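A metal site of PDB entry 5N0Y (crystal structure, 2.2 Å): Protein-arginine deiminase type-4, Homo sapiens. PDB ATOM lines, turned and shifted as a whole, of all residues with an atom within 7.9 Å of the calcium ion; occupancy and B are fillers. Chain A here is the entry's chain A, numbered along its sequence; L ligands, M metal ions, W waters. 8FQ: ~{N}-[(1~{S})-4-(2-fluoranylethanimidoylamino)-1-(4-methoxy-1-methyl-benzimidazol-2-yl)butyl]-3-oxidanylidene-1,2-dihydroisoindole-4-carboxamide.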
ATOM      1  N   MET A 305      16.086  -5.923  17.863  1.00  0.00           N
ATOM      2  CA  MET A 305      16.210  -4.479  18.164  1.00  0.00           C
ATOM      3  C   MET A 305      14.872  -3.819  18.387  1.00  0.00           C
ATOM      4  O   MET A 305      13.806  -4.362  18.029  1.00  0.00           O
ATOM      5  CB  MET A 305      16.861  -3.731  17.008  1.00  0.00           C
ATOM      6  CG  MET A 305      18.275  -4.115  16.791  1.00  0.00           C
ATOM      7  SD  MET A 305      19.040  -3.279  15.397  1.00  0.00           S
ATOM      8  CE  MET A 305      18.720  -1.566  15.821  1.00  0.00           C
ATOM      9  N   THR A 306      14.927  -2.596  18.922  1.00  0.00           N
ATOM     10  CA  THR A 306      13.719  -1.821  19.283  1.00  0.00           C
ATOM     11  C   THR A 306      13.795  -0.437  18.644  1.00  0.00           C
ATOM     12  O   THR A 306      14.742   0.321  18.917  1.00  0.00           O
ATOM     13  CB  THR A 306      13.574  -1.589  20.820  1.00  0.00           C
ATOM     14  OG1 THR A 306      14.729  -0.955  21.362  1.00  0.00           O
ATOM     15  CG2 THR A 306      13.349  -2.840  21.515  1.00  0.00           C
ATOM     16  N   ASN A 308      12.559   3.565  17.751  1.00  0.00           N
ATOM     17  CA  ASN A 308      12.333   4.791  18.480  1.00  0.00           C
ATOM     18  C   ASN A 308      10.875   4.980  18.954  1.00  0.00           C
ATOM     19  O   ASN A 308      10.611   5.797  19.846  1.00  0.00           O
ATOM     20  CB  ASN A 308      12.712   5.949  17.576  1.00  0.00           C
ATOM     21  CG  ASN A 308      14.180   6.088  17.382  1.00  0.00           C
ATOM     22  OD1 ASN A 308      14.999   5.341  17.952  1.00  0.00           O
ATOM     23  ND2 ASN A 308      14.550   7.042  16.536  1.00  0.00           N
ATOM     24  N   MET A 355      28.371   7.552  22.564  1.00  0.00           N
ATOM     25  CA  MET A 355      27.714   6.450  23.245  1.00  0.00           C
ATOM     26  C   MET A 355      26.766   5.640  22.315  1.00  0.00           C
ATOM     27  O   MET A 355      26.483   4.446  22.587  1.00  0.00           O
ATOM     28  CB  MET A 355      27.005   6.997  24.488  1.00  0.00           C
ATOM     29  CG  MET A 355      26.219   5.993  25.319  1.00  0.00           C
ATOM     30  SD  MET A 355      27.134   4.620  26.067  1.00  0.00           S
ATOM     31  CE  MET A 355      28.189   5.476  27.243  1.00  0.00           C
ATOM     32  N   GLN A 356      26.312   6.303  21.239  1.00  0.00           N
ATOM     33  CA  GLN A 356      25.548   5.693  20.158  1.00  0.00           C
ATOM     34  C   GLN A 356      26.319   4.624  19.411  1.00  0.00           C
ATOM     35  O   GLN A 356      25.750   3.670  18.895  1.00  0.00           O
ATOM     36  CB  GLN A 356      25.113   6.763  19.142  1.00  0.00           C
ATOM     37  CG  GLN A 356      24.322   6.278  17.900  1.00  0.00           C
ATOM     38  CD  GLN A 356      22.980   5.639  18.212  1.00  0.00           C
ATOM     39  OE1 GLN A 356      22.459   4.874  17.431  1.00  0.00           O
ATOM     40  NE2 GLN A 356      22.428   5.980  19.330  1.00  0.00           N
ATOM     41  N   ASP A 357      27.618   4.801  19.325  1.00  0.00           N
ATOM     42  CA  ASP A 357      28.361   4.097  18.304  1.00  0.00           C
ATOM     43  C   ASP A 357      28.926   2.725  18.701  1.00  0.00           C
ATOM     44  O   ASP A 357      29.151   1.864  17.807  1.00  0.00           O
ATOM     45  CB  ASP A 357      29.445   5.018  17.747  1.00  0.00           C
ATOM     46  CG  ASP A 357      28.861   6.121  16.836  1.00  0.00           C
ATOM     47  OD1 ASP A 357      27.696   5.938  16.341  1.00  0.00           O
ATOM     48  OD2 ASP A 357      29.554   7.156  16.629  1.00  0.00           O
ATOM     49  N   MET A 359      27.562   0.519  20.861  1.00  0.00           N
ATOM     50  CA  MET A 359      26.615  -0.523  21.237  1.00  0.00           C
ATOM     51  C   MET A 359      25.186  -0.340  20.738  1.00  0.00           C
ATOM     52  O   MET A 359      24.797   0.766  20.364  1.00  0.00           O
ATOM     53  CB  MET A 359      26.617  -0.645  22.753  1.00  0.00           C
ATOM     54  CG  MET A 359      25.786   0.348  23.502  1.00  0.00           C
ATOM     55  SD  MET A 359      26.092   0.256  25.299  1.00  0.00           S
ATOM     56  CE  MET A 359      24.754   1.303  25.883  1.00  0.00           C
ATOM     57  N   GLU A 360      24.416  -1.414  20.752  1.00  0.00           N
ATOM     58  CA  GLU A 360      22.972  -1.345  20.421  1.00  0.00           C
ATOM     59  C   GLU A 360      22.207  -2.246  21.370  1.00  0.00           C
ATOM     60  O   GLU A 360      22.594  -3.398  21.537  1.00  0.00           O
ATOM     61  CB  GLU A 360      22.727  -1.767  18.939  1.00  0.00           C
ATOM     62  CG  GLU A 360      21.286  -1.652  18.500  1.00  0.00           C
ATOM     63  CD  GLU A 360      20.831  -0.225  18.203  1.00  0.00           C
ATOM     64  OE1 GLU A 360      21.616   0.518  17.577  1.00  0.00           O
ATOM     65  OE2 GLU A 360      19.659   0.149  18.576  1.00  0.00           O
ATOM     66  N   ILE A 361      21.140  -1.741  21.989  1.00  0.00           N
ATOM     67  CA  ILE A 361      20.490  -2.532  23.012  1.00  0.00           C
ATOM     68  C   ILE A 361      19.254  -3.141  22.420  1.00  0.00           C
ATOM     69  O   ILE A 361      18.312  -2.409  22.120  1.00  0.00           O
ATOM     70  CB  ILE A 361      20.053  -1.782  24.301  1.00  0.00           C
ATOM     71  CG1 ILE A 361      21.141  -0.887  24.888  1.00  0.00           C
ATOM     72  CG2 ILE A 361      19.598  -2.795  25.346  1.00  0.00           C
ATOM     73  CD1 ILE A 361      22.448  -1.571  25.205  1.00  0.00           C
ATOM     74  N   SER A 413      30.014   1.186  13.149  1.00  0.00           N
ATOM     75  CA  SER A 413      29.569   1.907  14.343  1.00  0.00           C
ATOM     76  C   SER A 413      28.036   1.944  14.355  1.00  0.00           C
ATOM     77  O   SER A 413      27.399   2.022  13.282  1.00  0.00           O
ATOM     78  CB  SER A 413      30.143   3.339  14.348  1.00  0.00           C
ATOM     79  OG  SER A 413      31.584   3.363  14.370  1.00  0.00           O
ATOM     80  N   PHE A 414      27.426   1.861  15.540  1.00  0.00           N
ATOM     81  CA  PHE A 414      25.989   1.558  15.610  1.00  0.00           C
ATOM     82  C   PHE A 414      25.023   2.723  15.505  1.00  0.00           C
ATOM     83  O   PHE A 414      23.806   2.536  15.594  1.00  0.00           O
ATOM     84  CB  PHE A 414      25.674   0.631  16.752  1.00  0.00           C
ATOM     85  CG  PHE A 414      26.236  -0.780  16.583  1.00  0.00           C
ATOM     86  CD1 PHE A 414      26.906  -1.198  15.412  1.00  0.00           C
ATOM     87  CD2 PHE A 414      26.024  -1.715  17.593  1.00  0.00           C
ATOM     88  CE1 PHE A 414      27.354  -2.492  15.281  1.00  0.00           C
ATOM     89  CE2 PHE A 414      26.472  -3.031  17.465  1.00  0.00           C
ATOM     90  CZ  PHE A 414      27.145  -3.409  16.316  1.00  0.00           C
ATOM     91  N   GLY A 415      25.535   3.903  15.224  1.00  0.00           N
ATOM     92  CA  GLY A 415      24.693   4.931  14.682  1.00  0.00           C
ATOM     93  C   GLY A 415      24.323   4.573  13.249  1.00  0.00           C
ATOM     94  O   GLY A 415      23.419   5.217  12.656  1.00  0.00           O
ATOM     95  N   ASN A 416      25.044   3.611  12.664  1.00  0.00           N
ATOM     96  CA  ASN A 416      24.669   3.083  11.355  1.00  0.00           C
ATOM     97  C   ASN A 416      23.820   1.788  11.422  1.00  0.00           C
ATOM     98  O   ASN A 416      23.630   1.146  10.392  1.00  0.00           O
ATOM     99  CB  ASN A 416      25.920   2.821  10.541  1.00  0.00           C
ATOM    100  CG  ASN A 416      25.628   2.596   9.068  1.00  0.00           C
ATOM    101  OD1 ASN A 416      24.762   3.291   8.485  1.00  0.00           O
ATOM    102  ND2 ASN A 416      26.323   1.600   8.464  1.00  0.00           N
ATOM    103  N   LEU A 417      23.316   1.437  12.614  1.00  0.00           N
ATOM    104  CA  LEU A 417      22.387   0.366  12.827  1.00  0.00           C
ATOM    105  C   LEU A 417      21.114   0.894  13.491  1.00  0.00           C
ATOM    106  O   LEU A 417      21.174   1.371  14.610  1.00  0.00           O
ATOM    107  CB  LEU A 417      23.080  -0.667  13.702  1.00  0.00           C
ATOM    108  CG  LEU A 417      22.335  -1.925  14.071  1.00  0.00           C
ATOM    109  CD1 LEU A 417      21.751  -2.666  12.890  1.00  0.00           C
ATOM    110  CD2 LEU A 417      23.300  -2.792  14.816  1.00  0.00           C
ATOM    111  N   GLU A 418      19.987   0.835  12.776  1.00  0.00           N
ATOM    112  CA  GLU A 418      18.667   1.321  13.245  1.00  0.00           C
ATOM    113  C   GLU A 418      17.630   0.268  12.900  1.00  0.00           C
ATOM    114  O   GLU A 418      17.996  -0.805  12.436  1.00  0.00           O
ATOM    115  CB  GLU A 418      18.345   2.646  12.601  1.00  0.00           C
ATOM    116  CG  GLU A 418      19.367   3.739  12.965  1.00  0.00           C
ATOM    117  CD  GLU A 418      19.351   4.099  14.465  1.00  0.00           C
ATOM    118  OE1 GLU A 418      20.442   4.137  15.161  1.00  0.00           O
ATOM    119  OE2 GLU A 418      18.224   4.376  14.920  1.00  0.00           O
ATOM    120  N   VAL A 419      16.342   0.515  13.210  1.00  0.00           N
ATOM    121  CA  VAL A 419      15.220  -0.399  12.906  1.00  0.00           C
ATOM    122  C   VAL A 419      13.932   0.417  12.763  1.00  0.00           C
ATOM    123  O   VAL A 419      13.759   1.420  13.465  1.00  0.00           O
ATOM    124  CB  VAL A 419      15.069  -1.469  14.017  1.00  0.00           C
ATOM    125  CG1 VAL A 419      14.850  -0.879  15.401  1.00  0.00           C
ATOM    126  CG2 VAL A 419      13.977  -2.426  13.727  1.00  0.00           C
ATOM    127  N   LEU A 436      17.580  -1.462   9.542  1.00  0.00           N
ATOM    128  CA  LEU A 436      18.088  -0.612   8.504  1.00  0.00           C
ATOM    129  C   LEU A 436      19.551  -0.332   8.811  1.00  0.00           C
ATOM    130  O   LEU A 436      19.926  -0.014   9.959  1.00  0.00           O
ATOM    131  CB  LEU A 436      17.335   0.702   8.533  1.00  0.00           C
ATOM    132  CG  LEU A 436      15.826   0.656   8.535  1.00  0.00           C
ATOM    133  CD1 LEU A 436      15.289   2.034   8.911  1.00  0.00           C
ATOM    134  CD2 LEU A 436      15.338   0.163   7.184  1.00  0.00           C
ATOM    135  N   HIS A 478      26.494   7.348   8.474  1.00  0.00           N
ATOM    136  CA  HIS A 478      25.555   6.619   9.318  1.00  0.00           C
ATOM    137  C   HIS A 478      24.131   6.951   8.964  1.00  0.00           C
ATOM    138  O   HIS A 478      23.791   8.124   8.768  1.00  0.00           O
ATOM    139  CB  HIS A 478      25.780   7.011  10.754  1.00  0.00           C
ATOM    140  CG  HIS A 478      27.043   6.504  11.334  1.00  0.00           C
ATOM    141  ND1 HIS A 478      27.317   6.613  12.673  1.00  0.00           N
ATOM    142  CD2 HIS A 478      28.124   5.900  10.754  1.00  0.00           C
ATOM    143  CE1 HIS A 478      28.508   6.066  12.900  1.00  0.00           C
ATOM    144  NE2 HIS A 478      29.026   5.633  11.765  1.00  0.00           N
ATOM    145  N   VAL A 479      23.281   5.932   8.918  1.00  0.00           N
ATOM    146  CA  VAL A 479      21.860   6.209   8.643  1.00  0.00           C
ATOM    147  C   VAL A 479      21.206   7.163   9.654  1.00  0.00           C
ATOM    148  O   VAL A 479      20.317   7.892   9.256  1.00  0.00           O
ATOM    149  CB  VAL A 479      20.991   4.942   8.483  1.00  0.00           C
ATOM    150  CG1 VAL A 479      21.439   4.107   7.284  1.00  0.00           C
ATOM    151  CG2 VAL A 479      20.932   4.126   9.747  1.00  0.00           C
ATOM    152  N   ASP A 480      21.671   7.222  10.924  1.00  0.00           N
ATOM    153  CA  ASP A 480      21.102   8.198  11.877  1.00  0.00           C
ATOM    154  C   ASP A 480      21.400   9.651  11.470  1.00  0.00           C
ATOM    155  O   ASP A 480      20.764  10.589  11.915  1.00  0.00           O
ATOM    156  CB  ASP A 480      21.464   7.858  13.364  1.00  0.00           C
ATOM    157  CG  ASP A 480      22.940   8.215  13.783  1.00  0.00           C
ATOM    158  OD1 ASP A 480      23.784   8.514  12.901  1.00  0.00           O
ATOM    159  OD2 ASP A 480      23.244   8.266  15.045  1.00  0.00           O
ATOM    160  N   HIS A 651      21.878  12.521  19.139  1.00  0.00           N
ATOM    161  CA  HIS A 651      21.676  11.068  18.950  1.00  0.00           C
ATOM    162  C   HIS A 651      22.997  10.300  18.991  1.00  0.00           C
ATOM    163  O   HIS A 651      23.074   9.245  19.604  1.00  0.00           O
ATOM    164  CB  HIS A 651      20.891  10.726  17.668  1.00  0.00           C
ATOM    165  CG  HIS A 651      20.465   9.299  17.558  1.00  0.00           C
ATOM    166  ND1 HIS A 651      21.148   8.366  16.778  1.00  0.00           N
ATOM    167  CD2 HIS A 651      19.395   8.643  18.076  1.00  0.00           C
ATOM    168  CE1 HIS A 651      20.504   7.216  16.829  1.00  0.00           C
ATOM    169  NE2 HIS A 651      19.446   7.349  17.620  1.00  0.00           N
ATOM    170  N   THR A 654      24.339   9.797  22.657  1.00  0.00           N
ATOM    171  CA  THR A 654      23.437   9.045  23.565  1.00  0.00           C
ATOM    172  C   THR A 654      23.025   7.650  23.081  1.00  0.00           C
ATOM    173  O   THR A 654      23.321   7.273  21.965  1.00  0.00           O
ATOM    174  CB  THR A 654      22.147   9.823  23.790  1.00  0.00           C
ATOM    175  OG1 THR A 654      21.585  10.111  22.506  1.00  0.00           O
ATOM    176  CG2 THR A 654      22.453  11.122  24.520  1.00  0.00           C
ATOM    177  N   ASN A 655      22.346   6.895  23.958  1.00  0.00           N
ATOM    178  CA  ASN A 655      21.765   5.610  23.617  1.00  0.00           C
ATOM    179  C   ASN A 655      20.557   5.293  24.523  1.00  0.00           C
ATOM    180  O   ASN A 655      20.388   5.921  25.550  1.00  0.00           O
ATOM    181  CB  ASN A 655      22.840   4.499  23.645  1.00  0.00           C
ATOM    182  CG  ASN A 655      22.673   3.496  22.506  1.00  0.00           C
ATOM    183  OD1 ASN A 655      21.558   3.207  22.114  1.00  0.00           O
ATOM    184  ND2 ASN A 655      23.775   3.011  21.958  1.00  0.00           N
HETATM  185  C27 8FQ L   1      36.644  15.320  15.027  1.00  0.00           C
HETATM  186  C33 8FQ L   1      35.722   7.850  11.405  1.00  0.00           C
HETATM  187  C28 8FQ L   1      35.890  14.150  15.115  1.00  0.00           C
HETATM  188  C26 8FQ L   1      37.333  15.778  16.138  1.00  0.00           C
HETATM  189  C32 8FQ L   1      35.265   9.130  11.620  1.00  0.00           C
HETATM  190  C34 8FQ L   1      35.555   6.855  12.356  1.00  0.00           C
HETATM  191  C20 8FQ L   1      36.501  13.856  17.387  1.00  0.00           C
HETATM  192  C19 8FQ L   1      35.802  13.391  16.279  1.00  0.00           C
HETATM  193  C25 8FQ L   1      37.246  15.027  17.296  1.00  0.00           C
HETATM  194  C4  8FQ L   1      34.430   8.349  13.803  1.00  0.00           C
HETATM  195  C31 8FQ L   1      34.632   9.327  12.835  1.00  0.00           C
HETATM  196  C3  8FQ L   1      34.911   7.066  13.571  1.00  0.00           C
HETATM  197  C6  8FQ L   1      33.553  10.094  14.636  1.00  0.00           C
HETATM  198  C21 8FQ L   1      36.636  13.327  18.767  1.00  0.00           C
HETATM  199  C17 8FQ L   1      34.990  12.147  16.268  1.00  0.00           C
HETATM  200  C13 8FQ L   1      27.143   9.263  15.089  1.00  0.00           C
HETATM  201  C24 8FQ L   1      37.908  15.325  18.580  1.00  0.00           C
HETATM  202  C14 8FQ L   1      26.458  10.528  14.602  1.00  0.00           C
HETATM  203  C30 8FQ L   1      34.034  11.738  12.707  1.00  0.00           C
HETATM  204  C1  8FQ L   1      35.147   4.815  14.365  1.00  0.00           C
HETATM  205  C10 8FQ L   1      30.636  10.159  15.574  1.00  0.00           C
HETATM  206  C9  8FQ L   1      31.508  11.303  15.155  1.00  0.00           C
HETATM  207  C11 8FQ L   1      29.217  10.495  15.193  1.00  0.00           C
HETATM  208  C7  8FQ L   1      32.898  11.003  15.565  1.00  0.00           C
HETATM  209  N5  8FQ L   1      33.764   8.821  14.910  1.00  0.00           N
HETATM  210  N15 8FQ L   1      26.458   8.197  15.358  1.00  0.00           N
HETATM  211  N29 8FQ L   1      34.057  10.437  13.398  1.00  0.00           N
HETATM  212  N23 8FQ L   1      37.580  14.134  19.357  1.00  0.00           N
HETATM  213  N16 8FQ L   1      33.696  12.222  15.730  1.00  0.00           N
HETATM  214  N12 8FQ L   1      28.489   9.272  15.263  1.00  0.00           N
HETATM  215  O22 8FQ L   1      36.001  12.416  19.288  1.00  0.00           O
HETATM  216  O18 8FQ L   1      35.527  11.125  16.705  1.00  0.00           O
HETATM  217  O2  8FQ L   1      34.670   6.145  14.613  1.00  0.00           O
HETATM  218 CA    CA M   1      21.791   2.764  16.610  1.00  0.00          CA
HETATM  219  O   HOH W   1      19.497   2.755  17.743  1.00  0.00           O
HETATM  220  O   HOH W   2      23.469   2.526  18.612  1.00  0.00           O
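A ring nitrogen (ND1) of His 478 lies within hydrogen-bond range of a nitrogen (N15) of the ligand, at 3.2 Å. The side-chain carboxylate of Asp 480 lies within salt-bridge range of a nitrogen (N15) of the ligand, at 3.2 Å. OD2 of Asp 357 lies within salt-bridge range of N12 of the ligand (2.7 Å).
N of Phe 414 lies within hydrogen-bond range of O of Asp 357 (2.8 Å). The side-chain amide nitrogen (NE2) of Gln 356 sits close to the backbone carbonyl oxygen (O) of His 651, at 3.3 Å. The side-chain amide nitrogen (NE2) of Gln 356 sits at hydrogen-bond distance from the backbone carbonyl oxygen (O) of Thr 654. O of Leu 436 is in hydrogen-bond range of N of Glu 418 (2.9 Å).
Within 4 Å of the calcium ion: Gln 356, Glu 360, Phe 414, Leu 417 and Glu 418.
The calcium ion is bound by O of Phe 414, OE1 of Gln 356, OE1 of Glu 418, OE1 of Glu 360, O of Leu 417, water W1 and water W2. The calcium ion has seven donor atoms within binding distance.
Water W1 bridges the side-chain carboxylate (OE2) of Glu 360 (2.7 Å) and the side-chain carboxylate (OE2) of Glu 418 (3.5 Å). Water W2 lies within hydrogen-bond range of the backbone carbonyl oxygen (O) of Gln 356 (2.6 Å), the backbone carbonyl oxygen (O) of Met 359 (2.8 Å) and the side-chain amide nitrogen (ND2) of Asn 655 (3.4 Å).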
